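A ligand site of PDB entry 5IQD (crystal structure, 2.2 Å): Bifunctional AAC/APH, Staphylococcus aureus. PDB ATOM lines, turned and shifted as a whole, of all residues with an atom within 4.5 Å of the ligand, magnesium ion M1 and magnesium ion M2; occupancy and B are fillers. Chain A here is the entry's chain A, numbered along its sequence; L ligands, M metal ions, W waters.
OH of Tyr 100 lies within hydrogen-bond range of N3 of the ligand.
N of Ile 103 lies within hydrogen-bond range of O13 of the ligand (3.0 Å).
The backbone carbonyl oxygen (O) of Ile 103 is in hydrogen-bond range of a nitrogen (N4) of the ligand (2.9 Å).
The side-chain amino group (NZ) of Lys 52 lies within salt-bridge range of an oxygen (O7) of the ligand (2.9 Å).
An oxygen (O1) of the ligand sits at hydrogen-bond distance from the side-chain hydroxyl (OH) of Tyr 63 (2.9 Å).
OG of Ser 40 lies within hydrogen-bond range of N1 of the ligand.
The side-chain carboxylate of Asp 219 lies close to the side-chain amino group of Lys 52, 3.3 Å away.
N of Gly 221 lies close to OD1 of Asp 219 (3.2 Å).
N of Ile 218 is in hydrogen-bond range of O of His 205.
ND1 of His 205 lies within hydrogen-bond range of O of Asp 200.
The backbone carbonyl oxygen (O) of Tyr 100 lies within hydrogen-bond range of the backbone NH (N) of Ile 50 (2.7 Å).
The backbone carbonyl oxygen of Ala 42 is in hydrogen-bond range of the backbone NH of Ile 34 (3.0 Å).
N of Ala 42 lies within hydrogen-bond range of O of Gly 35, 2.7 Å away.
Merely in contact with the ligand: Phe 107 (3.4 Å), Ile 50 (3.6 Å), Ile 218 (3.6 Å), Glu 102 (3.6 Å), Ala 42 (3.7 Å), Ile 34 (3.8 Å) and Leu 207 (3.9 Å).
Hydrophobic or aromatic side chains within 4 Å of the ligand: Ile 34, Ala 42, Ile 50, Tyr 63, Tyr 100, Ile 103, Phe 107, His 205, Leu 207 and Ile 218.
14 residues have an atom within 4 Å of the ligand: Ile 34, Ser 40, Ala 42, Ile 50, Lys 52, Tyr 63, Tyr 100, Glu 102, Ile 103, Phe 107, His 205, Leu 207, Ile 218 and Asp 219.
Magnesium ion M1 is bound by water W4, O8 of the ligand, OD2 of Asp 219, water W7, O5 of the ligand and NE2 of His 205.
Magnesium ion M2 is bound by water W15 (2.0 Å), an oxygen (O3) of the ligand (2.0 Å), the side-chain carboxylate (OD2) of Asp 219 (2.1 Å), the side-chain carboxylate (OD1) of Asp 219 (2.1 Å), water W14 (2.2 Å) and water W11 (2.2 Å).
Magnesium ion M2 has six donor atoms within binding distance.
Water W3 lies within hydrogen-bond range of O7 of the ligand (2.7 Å), OH of Tyr 100 (2.8 Å) and N of Asp 219 (2.8 Å).
Water W1 lies within hydrogen-bond range of OG of Ser 40, O4 of the ligand, N of Ala 42 and N of Gly 37.
Water W13 lies within hydrogen-bond range of O of Ile 34 and O12 of the ligand.
Water W9 lies within hydrogen-bond range of the backbone carbonyl oxygen of Asn 204 (2.8 Å) and an oxygen (O11) of the ligand (3.0 Å).
Water W2 bridges the side-chain hydroxyl of Ser 40 (2.8 Å) and an oxygen (O2) of the ligand (3.3 Å).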
ATOM      1  N   ILE A  34      -2.241 -34.009 -19.830  1.00  0.00           N
ATOM      2  CA  ILE A  34      -2.625 -33.257 -18.603  1.00  0.00           C
ATOM      3  C   ILE A  34      -3.678 -32.202 -18.853  1.00  0.00           C
ATOM      4  O   ILE A  34      -4.214 -31.657 -17.921  1.00  0.00           O
ATOM      5  CB  ILE A  34      -1.507 -32.420 -17.999  1.00  0.00           C
ATOM      6  CG1 ILE A  34      -0.782 -31.776 -19.151  1.00  0.00           C
ATOM      7  CG2 ILE A  34      -0.671 -33.272 -17.109  1.00  0.00           C
ATOM      8  CD1 ILE A  34       0.469 -31.086 -18.807  1.00  0.00           C
ATOM      9  N   GLY A  35      -3.864 -31.843 -20.110  1.00  0.00           N
ATOM     10  CA  GLY A  35      -4.947 -30.938 -20.453  1.00  0.00           C
ATOM     11  C   GLY A  35      -5.220 -30.850 -21.939  1.00  0.00           C
ATOM     12  O   GLY A  35      -4.408 -31.258 -22.791  1.00  0.00           O
ATOM     13  N   SER A  36      -6.389 -30.320 -22.249  1.00  0.00           N
ATOM     14  CA  SER A  36      -6.771 -30.124 -23.633  1.00  0.00           C
ATOM     15  C   SER A  36      -7.794 -29.003 -23.752  1.00  0.00           C
ATOM     16  O   SER A  36      -8.567 -28.743 -22.830  1.00  0.00           O
ATOM     17  CB  SER A  36      -7.335 -31.395 -24.205  1.00  0.00           C
ATOM     18  OG  SER A  36      -8.616 -31.575 -23.688  1.00  0.00           O
ATOM     19  N   GLY A  37      -7.726 -28.287 -24.856  1.00  0.00           N
ATOM     20  CA  GLY A  37      -8.763 -27.326 -25.267  1.00  0.00           C
ATOM     21  C   GLY A  37      -9.493 -27.894 -26.469  1.00  0.00           C
ATOM     22  O   GLY A  37      -9.435 -29.124 -26.724  1.00  0.00           O
ATOM     23  N   SER A  40      -6.308 -27.849 -28.950  1.00  0.00           N
ATOM     24  CA  SER A  40      -4.984 -28.068 -28.485  1.00  0.00           C
ATOM     25  C   SER A  40      -4.940 -29.186 -27.460  1.00  0.00           C
ATOM     26  O   SER A  40      -5.948 -29.512 -26.813  1.00  0.00           O
ATOM     27  CB  SER A  40      -4.414 -26.799 -27.881  1.00  0.00           C
ATOM     28  OG  SER A  40      -5.001 -26.525 -26.613  1.00  0.00           O
ATOM     29  N   ALA A  42      -2.234 -30.571 -24.228  1.00  0.00           N
ATOM     30  CA  ALA A  42      -1.054 -30.421 -23.439  1.00  0.00           C
ATOM     31  C   ALA A  42      -0.652 -31.767 -22.806  1.00  0.00           C
ATOM     32  O   ALA A  42      -1.482 -32.481 -22.280  1.00  0.00           O
ATOM     33  CB  ALA A  42      -1.283 -29.356 -22.364  1.00  0.00           C
ATOM     34  N   ILE A  50       6.313 -29.793 -19.596  1.00  0.00           N
ATOM     35  CA  ILE A  50       5.016 -29.609 -20.250  1.00  0.00           C
ATOM     36  C   ILE A  50       5.281 -29.389 -21.729  1.00  0.00           C
ATOM     37  O   ILE A  50       6.147 -28.584 -22.101  1.00  0.00           O
ATOM     38  CB  ILE A  50       4.280 -28.353 -19.771  1.00  0.00           C
ATOM     39  CG1 ILE A  50       4.023 -28.384 -18.273  1.00  0.00           C
ATOM     40  CG2 ILE A  50       2.975 -28.166 -20.512  1.00  0.00           C
ATOM     41  CD1 ILE A  50       2.946 -29.347 -17.840  1.00  0.00           C
ATOM     42  N   LYS A  52       2.924 -28.149 -24.789  1.00  0.00           N
ATOM     43  CA  LYS A  52       1.689 -27.648 -25.350  1.00  0.00           C
ATOM     44  C   LYS A  52       1.720 -27.840 -26.872  1.00  0.00           C
ATOM     45  O   LYS A  52       2.691 -27.505 -27.475  1.00  0.00           O
ATOM     46  CB  LYS A  52       1.520 -26.143 -25.127  1.00  0.00           C
ATOM     47  CG  LYS A  52       1.056 -25.711 -23.787  1.00  0.00           C
ATOM     48  CD  LYS A  52       0.882 -24.199 -23.683  1.00  0.00           C
ATOM     49  CE  LYS A  52      -0.492 -23.732 -24.175  1.00  0.00           C
ATOM     50  NZ  LYS A  52      -0.820 -22.394 -23.605  1.00  0.00           N
ATOM     51  N   TYR A  63       0.886 -20.485 -31.831  1.00  0.00           N
ATOM     52  CA  TYR A  63       2.036 -20.513 -30.816  1.00  0.00           C
ATOM     53  C   TYR A  63       3.280 -19.625 -30.956  1.00  0.00           C
ATOM     54  O   TYR A  63       4.011 -19.424 -29.995  1.00  0.00           O
ATOM     55  CB  TYR A  63       2.480 -21.897 -30.338  1.00  0.00           C
ATOM     56  CG  TYR A  63       1.429 -22.679 -29.635  1.00  0.00           C
ATOM     57  CD1 TYR A  63       0.204 -22.113 -29.231  1.00  0.00           C
ATOM     58  CD2 TYR A  63       1.635 -24.010 -29.291  1.00  0.00           C
ATOM     59  CE1 TYR A  63      -0.743 -22.839 -28.579  1.00  0.00           C
ATOM     60  CE2 TYR A  63       0.661 -24.756 -28.651  1.00  0.00           C
ATOM     61  CZ  TYR A  63      -0.491 -24.170 -28.274  1.00  0.00           C
ATOM     62  OH  TYR A  63      -1.492 -24.875 -27.608  1.00  0.00           O
ATOM     63  N   TYR A 100       8.400 -26.706 -22.021  1.00  0.00           N
ATOM     64  CA  TYR A 100       9.046 -26.017 -20.918  1.00  0.00           C
ATOM     65  C   TYR A 100       8.955 -26.851 -19.671  1.00  0.00           C
ATOM     66  O   TYR A 100       8.114 -27.755 -19.593  1.00  0.00           O
ATOM     67  CB  TYR A 100       8.379 -24.664 -20.697  1.00  0.00           C
ATOM     68  CG  TYR A 100       6.867 -24.695 -20.479  1.00  0.00           C
ATOM     69  CD1 TYR A 100       6.335 -24.810 -19.236  1.00  0.00           C
ATOM     70  CD2 TYR A 100       5.993 -24.555 -21.557  1.00  0.00           C
ATOM     71  CE1 TYR A 100       4.954 -24.795 -19.039  1.00  0.00           C
ATOM     72  CE2 TYR A 100       4.625 -24.541 -21.381  1.00  0.00           C
ATOM     73  CZ  TYR A 100       4.093 -24.682 -20.127  1.00  0.00           C
ATOM     74  OH  TYR A 100       2.736 -24.677 -19.954  1.00  0.00           O
ATOM     75  N   LYS A 101       9.800 -26.558 -18.690  1.00  0.00           N
ATOM     76  CA  LYS A 101       9.714 -27.294 -17.443  1.00  0.00           C
ATOM     77  C   LYS A 101       8.426 -26.968 -16.701  1.00  0.00           C
ATOM     78  O   LYS A 101       8.061 -25.806 -16.543  1.00  0.00           O
ATOM     79  CB  LYS A 101      10.889 -27.007 -16.516  1.00  0.00           C
ATOM     80  CG  LYS A 101      12.201 -27.562 -17.049  1.00  0.00           C
ATOM     81  CD  LYS A 101      13.035 -28.160 -15.937  1.00  0.00           C
ATOM     82  CE  LYS A 101      14.364 -28.647 -16.471  1.00  0.00           C
ATOM     83  NZ  LYS A 101      15.270 -27.491 -16.760  1.00  0.00           N
ATOM     84  N   GLU A 102       7.757 -28.033 -16.258  1.00  0.00           N
ATOM     85  CA  GLU A 102       6.555 -27.947 -15.449  1.00  0.00           C
ATOM     86  C   GLU A 102       6.822 -27.089 -14.224  1.00  0.00           C
ATOM     87  O   GLU A 102       7.735 -27.361 -13.465  1.00  0.00           O
ATOM     88  CB  GLU A 102       6.130 -29.357 -14.957  1.00  0.00           C
ATOM     89  CG  GLU A 102       4.787 -29.403 -14.255  1.00  0.00           C
ATOM     90  CD  GLU A 102       4.575 -30.675 -13.446  1.00  0.00           C
ATOM     91  OE1 GLU A 102       5.528 -31.341 -13.133  1.00  0.00           O
ATOM     92  OE2 GLU A 102       3.441 -31.011 -13.060  1.00  0.00           O
ATOM     93  N   ILE A 103       5.979 -26.093 -13.983  1.00  0.00           N
ATOM     94  CA  ILE A 103       6.006 -25.379 -12.716  1.00  0.00           C
ATOM     95  C   ILE A 103       5.250 -26.190 -11.719  1.00  0.00           C
ATOM     96  O   ILE A 103       4.100 -26.587 -11.955  1.00  0.00           O
ATOM     97  CB  ILE A 103       5.364 -24.003 -12.845  1.00  0.00           C
ATOM     98  CG1 ILE A 103       6.148 -23.159 -13.836  1.00  0.00           C
ATOM     99  CG2 ILE A 103       5.368 -23.249 -11.498  1.00  0.00           C
ATOM    100  CD1 ILE A 103       5.398 -21.932 -14.307  1.00  0.00           C
ATOM    101  N   PHE A 107      -3.101 -25.962  -8.326  1.00  0.00           N
ATOM    102  CA  PHE A 107      -3.918 -24.914  -8.906  1.00  0.00           C
ATOM    103  C   PHE A 107      -4.905 -24.413  -7.911  1.00  0.00           C
ATOM    104  O   PHE A 107      -5.514 -25.183  -7.198  1.00  0.00           O
ATOM    105  CB  PHE A 107      -4.623 -25.342 -10.196  1.00  0.00           C
ATOM    106  CG  PHE A 107      -3.669 -25.378 -11.362  1.00  0.00           C
ATOM    107  CD1 PHE A 107      -3.175 -24.205 -11.897  1.00  0.00           C
ATOM    108  CD2 PHE A 107      -3.152 -26.585 -11.809  1.00  0.00           C
ATOM    109  CE1 PHE A 107      -2.286 -24.230 -12.955  1.00  0.00           C
ATOM    110  CE2 PHE A 107      -2.226 -26.619 -12.835  1.00  0.00           C
ATOM    111  CZ  PHE A 107      -1.789 -25.450 -13.400  1.00  0.00           C
ATOM    112  N   ASP A 200      -5.994 -13.982 -19.789  1.00  0.00           N
ATOM    113  CA  ASP A 200      -6.850 -15.184 -19.482  1.00  0.00           C
ATOM    114  C   ASP A 200      -6.642 -15.549 -18.004  1.00  0.00           C
ATOM    115  O   ASP A 200      -6.337 -16.690 -17.643  1.00  0.00           O
ATOM    116  CB  ASP A 200      -6.467 -16.340 -20.383  1.00  0.00           C
ATOM    117  CG  ASP A 200      -7.539 -17.372 -20.497  1.00  0.00           C
ATOM    118  OD1 ASP A 200      -8.674 -17.144 -20.024  1.00  0.00           O
ATOM    119  OD2 ASP A 200      -7.292 -18.407 -21.106  1.00  0.00           O
ATOM    120  N   ASN A 204      -7.722 -21.321 -12.661  1.00  0.00           N
ATOM    121  CA  ASN A 204      -7.110 -22.511 -13.222  1.00  0.00           C
ATOM    122  C   ASN A 204      -5.718 -22.255 -13.914  1.00  0.00           C
ATOM    123  O   ASN A 204      -5.116 -23.192 -14.430  1.00  0.00           O
ATOM    124  CB  ASN A 204      -8.058 -23.201 -14.172  1.00  0.00           C
ATOM    125  CG  ASN A 204      -8.242 -22.422 -15.462  1.00  0.00           C
ATOM    126  OD1 ASN A 204      -8.245 -21.216 -15.465  1.00  0.00           O
ATOM    127  ND2 ASN A 204      -8.313 -23.107 -16.555  1.00  0.00           N
ATOM    128  N   HIS A 205      -5.230 -21.013 -13.902  1.00  0.00           N
ATOM    129  CA  HIS A 205      -3.901 -20.703 -14.378  1.00  0.00           C
ATOM    130  C   HIS A 205      -3.013 -20.209 -13.270  1.00  0.00           C
ATOM    131  O   HIS A 205      -1.887 -19.813 -13.543  1.00  0.00           O
ATOM    132  CB  HIS A 205      -3.907 -19.683 -15.498  1.00  0.00           C
ATOM    133  CG  HIS A 205      -4.567 -20.164 -16.730  1.00  0.00           C
ATOM    134  ND1 HIS A 205      -5.342 -19.355 -17.532  1.00  0.00           N
ATOM    135  CD2 HIS A 205      -4.577 -21.384 -17.306  1.00  0.00           C
ATOM    136  CE1 HIS A 205      -5.793 -20.063 -18.567  1.00  0.00           C
ATOM    137  NE2 HIS A 205      -5.329 -21.300 -18.451  1.00  0.00           N
ATOM    138  N   LEU A 207      -0.946 -21.028  -9.713  1.00  0.00           N
ATOM    139  CA  LEU A 207      -0.394 -22.149  -8.931  1.00  0.00           C
ATOM    140  C   LEU A 207       0.037 -21.706  -7.565  1.00  0.00           C
ATOM    141  O   LEU A 207       0.652 -20.615  -7.375  1.00  0.00           O
ATOM    142  CB  LEU A 207       0.839 -22.747  -9.612  1.00  0.00           C
ATOM    143  CG  LEU A 207       0.507 -23.641 -10.794  1.00  0.00           C
ATOM    144  CD1 LEU A 207       1.659 -23.751 -11.740  1.00  0.00           C
ATOM    145  CD2 LEU A 207       0.103 -25.020 -10.318  1.00  0.00           C
ATOM    146  N   ILE A 218       0.566 -19.675 -15.414  1.00  0.00           N
ATOM    147  CA  ILE A 218       0.727 -20.330 -16.744  1.00  0.00           C
ATOM    148  C   ILE A 218      -0.218 -19.734 -17.780  1.00  0.00           C
ATOM    149  O   ILE A 218      -1.102 -18.932 -17.454  1.00  0.00           O
ATOM    150  CB  ILE A 218       0.484 -21.844 -16.673  1.00  0.00           C
ATOM    151  CG1 ILE A 218      -0.933 -22.167 -16.213  1.00  0.00           C
ATOM    152  CG2 ILE A 218       1.498 -22.492 -15.752  1.00  0.00           C
ATOM    153  CD1 ILE A 218      -1.348 -23.572 -16.564  1.00  0.00           C
ATOM    154  N   ASP A 219      -0.032 -20.194 -18.998  1.00  0.00           N
ATOM    155  CA  ASP A 219      -0.947 -19.924 -20.133  1.00  0.00           C
ATOM    156  C   ASP A 219      -1.106 -18.428 -20.442  1.00  0.00           C
ATOM    157  O   ASP A 219      -2.135 -17.845 -20.229  1.00  0.00           O
ATOM    158  CB  ASP A 219      -2.300 -20.568 -19.951  1.00  0.00           C
ATOM    159  CG  ASP A 219      -3.098 -20.606 -21.232  1.00  0.00           C
ATOM    160  OD1 ASP A 219      -2.604 -20.013 -22.223  1.00  0.00           O
ATOM    161  OD2 ASP A 219      -4.224 -21.197 -21.266  1.00  0.00           O
ATOM    162  N   GLY A 221      -1.012 -17.537 -23.412  1.00  0.00           N
ATOM    163  CA  GLY A 221      -1.337 -17.702 -24.785  1.00  0.00           C
ATOM    164  C   GLY A 221      -2.229 -16.616 -25.345  1.00  0.00           C
ATOM    165  O   GLY A 221      -2.299 -16.459 -26.559  1.00  0.00           O
HETATM  166  P1  LIG L   1      -4.295 -22.918 -25.305  1.00  0.00           P
HETATM  167  O1  LIG L   1      -3.589 -23.132 -26.578  1.00  0.00           O
HETATM  168  O2  LIG L   1      -5.890 -22.610 -25.738  1.00  0.00           O
HETATM  169  O3  LIG L   1      -3.632 -21.880 -24.320  1.00  0.00           O
HETATM  170  N1  LIG L   1      -4.263 -24.340 -24.516  1.00  0.00           N
HETATM  171  P2  LIG L   1      -4.615 -24.632 -22.968  1.00  0.00           P
HETATM  172  O4  LIG L   1      -5.242 -25.940 -22.738  1.00  0.00           O
HETATM  173  O5  LIG L   1      -5.637 -23.388 -22.383  1.00  0.00           O
HETATM  174  O6  LIG L   1      -3.236 -24.497 -22.296  1.00  0.00           O
HETATM  175  P3  LIG L   1      -2.585 -24.395 -20.848  1.00  0.00           P
HETATM  176  O7  LIG L   1      -1.390 -23.523 -20.990  1.00  0.00           O
HETATM  177  O8  LIG L   1      -3.556 -23.751 -19.876  1.00  0.00           O
HETATM  178  O9  LIG L   1      -2.180 -25.822 -20.207  1.00  0.00           O
HETATM  179  C1  LIG L   1      -3.075 -26.906 -20.182  1.00  0.00           C
HETATM  180  C2  LIG L   1      -3.059 -27.463 -18.789  1.00  0.00           C
HETATM  181  O10 LIG L   1      -1.797 -28.104 -18.530  1.00  0.00           O
HETATM  182  C3  LIG L   1      -3.253 -26.496 -17.632  1.00  0.00           C
HETATM  183  O11 LIG L   1      -4.638 -26.406 -17.281  1.00  0.00           O
HETATM  184  C4  LIG L   1      -2.596 -27.266 -16.495  1.00  0.00           C
HETATM  185  O12 LIG L   1      -3.359 -28.412 -16.219  1.00  0.00           O
HETATM  186  C5  LIG L   1      -1.398 -27.903 -17.198  1.00  0.00           C
HETATM  187  N2  LIG L   1      -0.170 -27.123 -17.168  1.00  0.00           N
HETATM  188  C6  LIG L   1       0.451 -26.422 -18.175  1.00  0.00           C
HETATM  189  N3  LIG L   1       1.562 -25.827 -17.800  1.00  0.00           N
HETATM  190  C7  LIG L   1       1.676 -26.172 -16.467  1.00  0.00           C
HETATM  191  C8  LIG L   1       2.716 -25.946 -15.560  1.00  0.00           C
HETATM  192  O13 LIG L   1       3.740 -25.305 -15.768  1.00  0.00           O
HETATM  193  N4  LIG L   1       2.507 -26.559 -14.349  1.00  0.00           N
HETATM  194  C9  LIG L   1       1.436 -27.336 -14.041  1.00  0.00           C
HETATM  195  N5  LIG L   1       1.368 -27.815 -12.799  1.00  0.00           N
HETATM  196  N6  LIG L   1       0.451 -27.579 -14.895  1.00  0.00           N
HETATM  197  C10 LIG L   1       0.626 -26.961 -16.075  1.00  0.00           C
HETATM  198 MG    MG M   1      -5.222 -22.711 -20.299  1.00  0.00          MG
HETATM  199 MG    MG M   2      -4.453 -20.401 -23.213  1.00  0.00          MG
HETATM  200  O   HOH W   1      -4.291 -27.878 -24.421  1.00  0.00           O
HETATM  201  O   HOH W   2      -7.095 -25.014 -27.577  1.00  0.00           O
HETATM  202  O   HOH W   3       0.975 -22.528 -20.257  1.00  0.00           O
HETATM  203  O   HOH W   4      -6.391 -23.930 -19.451  1.00  0.00           O
HETATM  204  O   HOH W   5      -0.637 -29.587 -10.836  1.00  0.00           O
HETATM  205  O   HOH W   6      -6.976 -26.438 -20.663  1.00  0.00           O
HETATM  206  O   HOH W   7      -6.956 -21.922 -21.248  1.00  0.00           O
HETATM  207  O   HOH W   8      -2.117 -20.404 -27.040  1.00  0.00           O
HETATM  208  O   HOH W   9      -5.459 -25.963 -14.391  1.00  0.00           O
HETATM  209  O   HOH W  10      -1.042 -30.340 -13.349  1.00  0.00           O
HETATM  210  O   HOH W  11      -5.101 -18.379 -22.637  1.00  0.00           O
HETATM  211  O   HOH W  12      -5.109 -23.175 -28.511  1.00  0.00           O
HETATM  212  O   HOH W  13      -5.902 -29.318 -17.405  1.00  0.00           O
HETATM  213  O   HOH W  14      -4.078 -19.311 -25.030  1.00  0.00           O
HETATM  214  O   HOH W  15      -6.285 -20.847 -23.765  1.00  0.00           O
